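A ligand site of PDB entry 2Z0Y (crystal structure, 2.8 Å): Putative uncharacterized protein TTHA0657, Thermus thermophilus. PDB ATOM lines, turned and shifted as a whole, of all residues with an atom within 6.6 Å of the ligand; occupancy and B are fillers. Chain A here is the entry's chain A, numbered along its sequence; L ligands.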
ATOM      1  N   VAL A 157     -10.377  21.950  -5.722  1.00  0.00           N
ATOM      2  CA  VAL A 157     -11.402  21.126  -6.336  1.00  0.00           C
ATOM      3  C   VAL A 157     -10.998  19.659  -6.323  1.00  0.00           C
ATOM      4  O   VAL A 157     -10.057  19.259  -7.003  1.00  0.00           O
ATOM      5  CB  VAL A 157     -11.683  21.571  -7.792  1.00  0.00           C
ATOM      6  CG1 VAL A 157     -10.396  21.570  -8.602  1.00  0.00           C
ATOM      7  CG2 VAL A 157     -12.707  20.633  -8.425  1.00  0.00           C
ATOM      8  N   ALA A 158     -11.713  18.866  -5.531  1.00  0.00           N
ATOM      9  CA  ALA A 158     -11.419  17.446  -5.455  1.00  0.00           C
ATOM     10  C   ALA A 158     -11.561  16.858  -6.856  1.00  0.00           C
ATOM     11  O   ALA A 158     -12.667  16.721  -7.367  1.00  0.00           O
ATOM     12  CB  ALA A 158     -12.398  16.756  -4.491  1.00  0.00           C
ATOM     13  N   HIS A 159     -10.433  16.539  -7.478  1.00  0.00           N
ATOM     14  CA  HIS A 159     -10.460  15.997  -8.823  1.00  0.00           C
ATOM     15  C   HIS A 159      -9.719  14.671  -8.922  1.00  0.00           C
ATOM     16  O   HIS A 159      -8.514  14.599  -8.678  1.00  0.00           O
ATOM     17  CB  HIS A 159      -9.835  17.001  -9.802  1.00  0.00           C
ATOM     18  CG  HIS A 159      -9.996  16.615 -11.239  1.00  0.00           C
ATOM     19  ND1 HIS A 159     -11.234  16.425 -11.823  1.00  0.00           N
ATOM     20  CD2 HIS A 159      -9.080  16.367 -12.210  1.00  0.00           C
ATOM     21  CE1 HIS A 159     -11.065  16.082 -13.091  1.00  0.00           C
ATOM     22  NE2 HIS A 159      -9.774  16.046 -13.343  1.00  0.00           N
ATOM     23  N   VAL A 160     -10.448  13.612  -9.280  1.00  0.00           N
ATOM     24  CA  VAL A 160      -9.855  12.288  -9.411  1.00  0.00           C
ATOM     25  C   VAL A 160      -8.594  12.343 -10.261  1.00  0.00           C
ATOM     26  O   VAL A 160      -7.628  11.617  -9.996  1.00  0.00           O
ATOM     27  CB  VAL A 160     -10.836  11.304 -10.066  1.00  0.00           C
ATOM     28  CG1 VAL A 160     -10.217   9.913 -10.114  1.00  0.00           C
ATOM     29  CG2 VAL A 160     -12.139  11.267  -9.286  1.00  0.00           C
ATOM     30  N   GLY A 161      -8.605  13.191 -11.280  1.00  0.00           N
ATOM     31  CA  GLY A 161      -7.455  13.316 -12.152  1.00  0.00           C
ATOM     32  C   GLY A 161      -6.516  14.434 -11.748  1.00  0.00           C
ATOM     33  O   GLY A 161      -6.379  15.425 -12.474  1.00  0.00           O
ATOM     34  N   ALA A 162      -5.875  14.291 -10.589  1.00  0.00           N
ATOM     35  CA  ALA A 162      -4.950  15.304 -10.099  1.00  0.00           C
ATOM     36  C   ALA A 162      -3.725  14.638  -9.475  1.00  0.00           C
ATOM     37  O   ALA A 162      -3.714  13.434  -9.247  1.00  0.00           O
ATOM     38  CB  ALA A 162      -5.639  16.185  -9.071  1.00  0.00           C
ATOM     39  N   ALA A 179     -14.692  22.398  -3.922  1.00  0.00           N
ATOM     40  CA  ALA A 179     -15.587  21.991  -4.993  1.00  0.00           C
ATOM     41  C   ALA A 179     -15.550  20.492  -5.224  1.00  0.00           C
ATOM     42  O   ALA A 179     -14.495  19.902  -5.436  1.00  0.00           O
ATOM     43  CB  ALA A 179     -15.224  22.726  -6.269  1.00  0.00           C
ATOM     44  N   VAL A 180     -16.731  19.875  -5.171  1.00  0.00           N
ATOM     45  CA  VAL A 180     -16.870  18.433  -5.383  1.00  0.00           C
ATOM     46  C   VAL A 180     -17.843  18.203  -6.539  1.00  0.00           C
ATOM     47  O   VAL A 180     -18.799  18.955  -6.703  1.00  0.00           O
ATOM     48  CB  VAL A 180     -17.414  17.728  -4.123  1.00  0.00           C
ATOM     49  CG1 VAL A 180     -17.390  16.226  -4.328  1.00  0.00           C
ATOM     50  CG2 VAL A 180     -16.594  18.117  -2.904  1.00  0.00           C
ATOM     51  N   GLY A 181     -17.604  17.157  -7.319  1.00  0.00           N
ATOM     52  CA  GLY A 181     -18.465  16.850  -8.445  1.00  0.00           C
ATOM     53  C   GLY A 181     -19.607  15.921  -8.081  1.00  0.00           C
ATOM     54  O   GLY A 181     -19.487  15.147  -7.129  1.00  0.00           O
ATOM     55  N   PRO A 182     -20.717  15.956  -8.832  1.00  0.00           N
ATOM     56  CA  PRO A 182     -21.884  15.094  -8.565  1.00  0.00           C
ATOM     57  C   PRO A 182     -21.548  13.617  -8.667  1.00  0.00           C
ATOM     58  O   PRO A 182     -20.379  13.241  -8.799  1.00  0.00           O
ATOM     59  CB  PRO A 182     -22.879  15.543  -9.625  1.00  0.00           C
ATOM     60  CG  PRO A 182     -21.998  15.897 -10.778  1.00  0.00           C
ATOM     61  CD  PRO A 182     -20.895  16.694 -10.097  1.00  0.00           C
ATOM     62  N   GLU A 183     -22.575  12.763  -8.611  1.00  0.00           N
ATOM     63  CA  GLU A 183     -22.374  11.327  -8.702  1.00  0.00           C
ATOM     64  C   GLU A 183     -21.613  10.985  -9.976  1.00  0.00           C
ATOM     65  O   GLU A 183     -20.798  10.062  -9.996  1.00  0.00           O
ATOM     66  CB  GLU A 183     -23.725  10.599  -8.682  1.00  0.00           C
ATOM     67  CG  GLU A 183     -24.463  10.696  -7.357  1.00  0.00           C
ATOM     68  CD  GLU A 183     -25.324  11.940  -7.251  1.00  0.00           C
ATOM     69  OE1 GLU A 183     -24.932  12.995  -7.775  1.00  0.00           O
ATOM     70  OE2 GLU A 183     -26.406  11.853  -6.627  1.00  0.00           O
ATOM     71  N   GLY A 184     -21.872  11.760 -11.031  1.00  0.00           N
ATOM     72  CA  GLY A 184     -21.183  11.544 -12.287  1.00  0.00           C
ATOM     73  C   GLY A 184     -19.818  12.208 -12.219  1.00  0.00           C
ATOM     74  O   GLY A 184     -18.800  11.623 -12.592  1.00  0.00           O
ATOM     75  N   GLY A 185     -19.806  13.447 -11.740  1.00  0.00           N
ATOM     76  CA  GLY A 185     -18.564  14.190 -11.617  1.00  0.00           C
ATOM     77  C   GLY A 185     -18.529  15.436 -12.476  1.00  0.00           C
ATOM     78  O   GLY A 185     -19.458  15.703 -13.238  1.00  0.00           O
ATOM     79  N   PHE A 186     -17.459  16.206 -12.347  1.00  0.00           N
ATOM     80  CA  PHE A 186     -17.285  17.426 -13.123  1.00  0.00           C
ATOM     81  C   PHE A 186     -16.833  17.059 -14.527  1.00  0.00           C
ATOM     82  O   PHE A 186     -16.042  16.138 -14.714  1.00  0.00           O
ATOM     83  CB  PHE A 186     -16.241  18.329 -12.458  1.00  0.00           C
ATOM     84  CG  PHE A 186     -16.773  19.119 -11.288  1.00  0.00           C
ATOM     85  CD1 PHE A 186     -15.924  19.485 -10.244  1.00  0.00           C
ATOM     86  CD2 PHE A 186     -18.101  19.514 -11.241  1.00  0.00           C
ATOM     87  CE1 PHE A 186     -16.397  20.237  -9.172  1.00  0.00           C
ATOM     88  CE2 PHE A 186     -18.583  20.262 -10.171  1.00  0.00           C
ATOM     89  CZ  PHE A 186     -17.731  20.621  -9.132  1.00  0.00           C
ATOM     90  N   VAL A 202      -7.063  18.820  -6.707  1.00  0.00           N
ATOM     91  CA  VAL A 202      -6.485  18.092  -5.585  1.00  0.00           C
ATOM     92  C   VAL A 202      -6.960  16.646  -5.568  1.00  0.00           C
ATOM     93  O   VAL A 202      -8.111  16.360  -5.932  1.00  0.00           O
ATOM     94  CB  VAL A 202      -6.828  18.754  -4.232  1.00  0.00           C
ATOM     95  CG1 VAL A 202      -6.146  20.096  -4.114  1.00  0.00           C
ATOM     96  CG2 VAL A 202      -8.344  18.910  -4.095  1.00  0.00           C
ATOM     97  N   SER A 203      -6.085  15.746  -5.154  1.00  0.00           N
ATOM     98  CA  SER A 203      -6.407  14.331  -5.075  1.00  0.00           C
ATOM     99  C   SER A 203      -6.848  13.932  -3.667  1.00  0.00           C
ATOM    100  O   SER A 203      -6.338  14.440  -2.668  1.00  0.00           O
ATOM    101  CB  SER A 203      -5.185  13.503  -5.475  1.00  0.00           C
ATOM    102  OG  SER A 203      -5.390  12.121  -5.219  1.00  0.00           O
ATOM    103  N   LEU A 204      -7.822  13.022  -3.603  1.00  0.00           N
ATOM    104  CA  LEU A 204      -8.321  12.532  -2.328  1.00  0.00           C
ATOM    105  C   LEU A 204      -8.046  11.039  -2.216  1.00  0.00           C
ATOM    106  O   LEU A 204      -8.873  10.283  -1.703  1.00  0.00           O
ATOM    107  CB  LEU A 204      -9.828  12.781  -2.207  1.00  0.00           C
ATOM    108  CG  LEU A 204     -10.297  14.233  -2.084  1.00  0.00           C
ATOM    109  CD1 LEU A 204     -11.817  14.265  -1.974  1.00  0.00           C
ATOM    110  CD2 LEU A 204      -9.663  14.886  -0.866  1.00  0.00           C
ATOM    111  N   GLY A 205      -6.894  10.623  -2.727  1.00  0.00           N
ATOM    112  CA  GLY A 205      -6.528   9.220  -2.678  1.00  0.00           C
ATOM    113  C   GLY A 205      -6.570   8.552  -4.036  1.00  0.00           C
ATOM    114  O   GLY A 205      -6.836   9.192  -5.046  1.00  0.00           O
ATOM    115  N   ARG A 206      -6.339   7.238  -4.041  1.00  0.00           N
ATOM    116  CA  ARG A 206      -6.332   6.460  -5.277  1.00  0.00           C
ATOM    117  C   ARG A 206      -7.573   5.593  -5.467  1.00  0.00           C
ATOM    118  O   ARG A 206      -7.547   4.620  -6.219  1.00  0.00           O
ATOM    119  CB  ARG A 206      -5.066   5.605  -5.321  1.00  0.00           C
ATOM    120  CG  ARG A 206      -3.787   6.423  -5.395  1.00  0.00           C
ATOM    121  CD  ARG A 206      -2.539   5.583  -5.235  1.00  0.00           C
ATOM    122  NE  ARG A 206      -2.399   5.056  -3.873  1.00  0.00           N
ATOM    123  CZ  ARG A 206      -1.306   4.450  -3.424  1.00  0.00           C
ATOM    124  NH1 ARG A 206      -0.259   4.286  -4.217  1.00  0.00           N
ATOM    125  NH2 ARG A 206      -1.258   4.002  -2.175  1.00  0.00           N
ATOM    126  N   ARG A 207      -8.650   5.957  -4.790  1.00  0.00           N
ATOM    127  CA  ARG A 207      -9.908   5.219  -4.879  1.00  0.00           C
ATOM    128  C   ARG A 207     -11.053   6.171  -5.178  1.00  0.00           C
ATOM    129  O   ARG A 207     -11.025   7.329  -4.759  1.00  0.00           O
ATOM    130  CB  ARG A 207     -10.198   4.483  -3.579  1.00  0.00           C
ATOM    131  CG  ARG A 207      -9.241   3.364  -3.249  1.00  0.00           C
ATOM    132  CD  ARG A 207      -9.247   3.095  -1.754  1.00  0.00           C
ATOM    133  NE  ARG A 207      -8.827   4.292  -1.024  1.00  0.00           N
ATOM    134  CZ  ARG A 207      -7.604   4.796  -1.077  1.00  0.00           C
ATOM    135  NH1 ARG A 207      -6.672   4.207  -1.810  1.00  0.00           N
ATOM    136  NH2 ARG A 207      -7.318   5.909  -0.404  1.00  0.00           N
ATOM    137  N   ILE A 208     -12.065   5.678  -5.883  1.00  0.00           N
ATOM    138  CA  ILE A 208     -13.225   6.485  -6.224  1.00  0.00           C
ATOM    139  C   ILE A 208     -14.002   6.754  -4.944  1.00  0.00           C
ATOM    140  O   ILE A 208     -14.206   5.857  -4.136  1.00  0.00           O
ATOM    141  CB  ILE A 208     -14.148   5.757  -7.205  1.00  0.00           C
ATOM    142  CG1 ILE A 208     -13.316   5.090  -8.306  1.00  0.00           C
ATOM    143  CG2 ILE A 208     -15.118   6.744  -7.833  1.00  0.00           C
ATOM    144  CD1 ILE A 208     -14.108   4.124  -9.173  1.00  0.00           C
ATOM    145  N   LEU A 209     -14.452   7.998  -4.765  1.00  0.00           N
ATOM    146  CA  LEU A 209     -15.194   8.341  -3.560  1.00  0.00           C
ATOM    147  C   LEU A 209     -16.520   9.013  -3.890  1.00  0.00           C
ATOM    148  O   LEU A 209     -16.599   9.836  -4.795  1.00  0.00           O
ATOM    149  CB  LEU A 209     -14.362   9.279  -2.673  1.00  0.00           C
ATOM    150  CG  LEU A 209     -12.974   8.782  -2.248  1.00  0.00           C
ATOM    151  CD1 LEU A 209     -12.272   9.862  -1.437  1.00  0.00           C
ATOM    152  CD2 LEU A 209     -13.119   7.505  -1.445  1.00  0.00           C
ATOM    153  N   ARG A 210     -17.558   8.656  -3.134  1.00  0.00           N
ATOM    154  CA  ARG A 210     -18.867   9.251  -3.345  1.00  0.00           C
ATOM    155  C   ARG A 210     -18.763  10.749  -3.117  1.00  0.00           C
ATOM    156  O   ARG A 210     -17.897  11.220  -2.387  1.00  0.00           O
ATOM    157  CB  ARG A 210     -19.870   8.644  -2.358  1.00  0.00           C
ATOM    158  CG  ARG A 210     -20.059   7.150  -2.511  1.00  0.00           C
ATOM    159  CD  ARG A 210     -20.972   6.620  -1.436  1.00  0.00           C
ATOM    160  NE  ARG A 210     -20.320   6.575  -0.128  1.00  0.00           N
ATOM    161  CZ  ARG A 210     -20.971   6.579   1.031  1.00  0.00           C
ATOM    162  NH1 ARG A 210     -22.286   6.636   1.052  1.00  0.00           N
ATOM    163  NH2 ARG A 210     -20.293   6.517   2.172  1.00  0.00           N
ATOM    164  N   ALA A 211     -19.637  11.515  -3.756  1.00  0.00           N
ATOM    165  CA  ALA A 211     -19.626  12.972  -3.610  1.00  0.00           C
ATOM    166  C   ALA A 211     -19.628  13.383  -2.145  1.00  0.00           C
ATOM    167  O   ALA A 211     -18.979  14.362  -1.759  1.00  0.00           O
ATOM    168  CB  ALA A 211     -20.836  13.570  -4.323  1.00  0.00           C
ATOM    169  N   GLU A 212     -20.352  12.634  -1.326  1.00  0.00           N
ATOM    170  CA  GLU A 212     -20.434  12.928   0.096  1.00  0.00           C
ATOM    171  C   GLU A 212     -19.104  12.670   0.794  1.00  0.00           C
ATOM    172  O   GLU A 212     -18.601  13.534   1.514  1.00  0.00           O
ATOM    173  CB  GLU A 212     -21.531  12.075   0.757  1.00  0.00           C
ATOM    174  CG  GLU A 212     -22.909  12.238   0.133  1.00  0.00           C
ATOM    175  CD  GLU A 212     -23.206  11.191  -0.934  1.00  0.00           C
ATOM    176  OE1 GLU A 212     -22.493  11.158  -1.971  1.00  0.00           O
ATOM    177  OE2 GLU A 212     -24.147  10.409  -0.741  1.00  0.00           O
ATOM    178  N   ALA A 214     -16.325  12.607  -0.520  1.00  0.00           N
ATOM    179  CA  ALA A 214     -15.363  13.513  -1.120  1.00  0.00           C
ATOM    180  C   ALA A 214     -15.385  14.867  -0.442  1.00  0.00           C
ATOM    181  O   ALA A 214     -14.324  15.446  -0.167  1.00  0.00           O
ATOM    182  CB  ALA A 214     -15.673  13.673  -2.602  1.00  0.00           C
ATOM    183  N   ALA A 215     -16.578  15.385  -0.195  1.00  0.00           N
ATOM    184  CA  ALA A 215     -16.737  16.679   0.461  1.00  0.00           C
ATOM    185  C   ALA A 215     -16.220  16.615   1.888  1.00  0.00           C
ATOM    186  O   ALA A 215     -15.658  17.585   2.405  1.00  0.00           O
ATOM    187  CB  ALA A 215     -18.197  17.103   0.441  1.00  0.00           C
HETATM  188  N1  LIG L   1     -15.426  10.728 -11.755  1.00  0.00           N
HETATM  189  C1  LIG L   1     -15.589   9.581 -10.850  1.00  0.00           C
HETATM  190  C2  LIG L   1     -14.940   8.349 -11.490  1.00  0.00           C
HETATM  191  O1  LIG L   1     -15.328   8.049 -12.643  1.00  0.00           O
HETATM  192  O2  LIG L   1     -14.080   7.748 -10.813  1.00  0.00           O
HETATM  193  C3  LIG L   1     -17.070   9.327 -10.608  1.00  0.00           C
HETATM  194  C4  LIG L   1     -17.758  10.557 -10.001  1.00  0.00           C
HETATM  195  S1  LIG L   1     -17.045  11.084  -8.400  1.00  0.00           S
HETATM  196  C5  LIG L   1     -17.780   9.864  -7.330  1.00  0.00           C
HETATM  197  C6  LIG L   1     -17.855  12.608  -7.794  1.00  0.00           C
HETATM  198  C7  LIG L   1     -16.897  13.551  -7.077  1.00  0.00           C
HETATM  199  O3  LIG L   1     -16.289  12.958  -5.912  1.00  0.00           O
HETATM  200  C8  LIG L   1     -15.699  13.897  -7.970  1.00  0.00           C
HETATM  201  O4  LIG L   1     -16.119  14.869  -8.928  1.00  0.00           O
HETATM  202  C9  LIG L   1     -14.837  14.563  -6.909  1.00  0.00           C
HETATM  203  O5  LIG L   1     -15.402  15.829  -6.552  1.00  0.00           O
HETATM  204  C10 LIG L   1     -14.995  13.579  -5.745  1.00  0.00           C
HETATM  205  N2  LIG L   1     -13.981  12.515  -5.808  1.00  0.00           N
HETATM  206  C11 LIG L   1     -14.209  11.202  -5.756  1.00  0.00           C
HETATM  207  N3  LIG L   1     -13.054  10.536  -5.747  1.00  0.00           N
HETATM  208  C12 LIG L   1     -12.076  11.433  -5.797  1.00  0.00           C
HETATM  209  C13 LIG L   1     -10.689  11.351  -5.801  1.00  0.00           C
HETATM  210  N4  LIG L   1     -10.087  10.166  -5.721  1.00  0.00           N
HETATM  211  N5  LIG L   1      -9.972  12.483  -5.859  1.00  0.00           N
HETATM  212  C14 LIG L   1     -10.566  13.665  -5.903  1.00  0.00           C
HETATM  213  N6  LIG L   1     -11.881  13.781  -5.898  1.00  0.00           N
HETATM  214  C15 LIG L   1     -12.658  12.695  -5.841  1.00  0.00           C
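An oxygen (O5) of the ligand sits at hydrogen-bond distance from the backbone NH (N) of Gly 181, at 2.7 Å. A nitrogen (N3) of the ligand lies within hydrogen-bond range of the backbone NH of Leu 209. O5 of the ligand lies within hydrogen-bond range of O of Ala 158. The backbone carbonyl oxygen (O) of Arg 207 sits at hydrogen-bond distance from a nitrogen (N4) of the ligand (3.1 Å). The backbone NH (N) of Leu 204 lies within hydrogen-bond range of a nitrogen (N5) of the ligand. N6 of the ligand sits close to N of His 159 (3.5 Å). The backbone carbonyl oxygen of Gly 205 is in hydrogen-bond range of a nitrogen (N4) of the ligand (3.5 Å).
O of Ala 179 lies within hydrogen-bond range of N of Ala 158 (3.0 Å). O of Val 202 sits at hydrogen-bond distance from N of His 159. The backbone carbonyl oxygen (O) of Gly 205 is in hydrogen-bond range of the side-chain hydroxyl (OG) of Ser 203 (3.3 Å). The backbone NH (N) of Val 202 lies within hydrogen-bond range of the backbone carbonyl oxygen (O) of Val 157.
Merely in contact with the ligand: Pro 182, Gly 184, Val 180, Glu 183, Ala 214, Ile 208, Val 160, Val 202, Gly 185 and Phe 186. Of the 27 residues printed, 17 come within 4 Å of the ligand.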
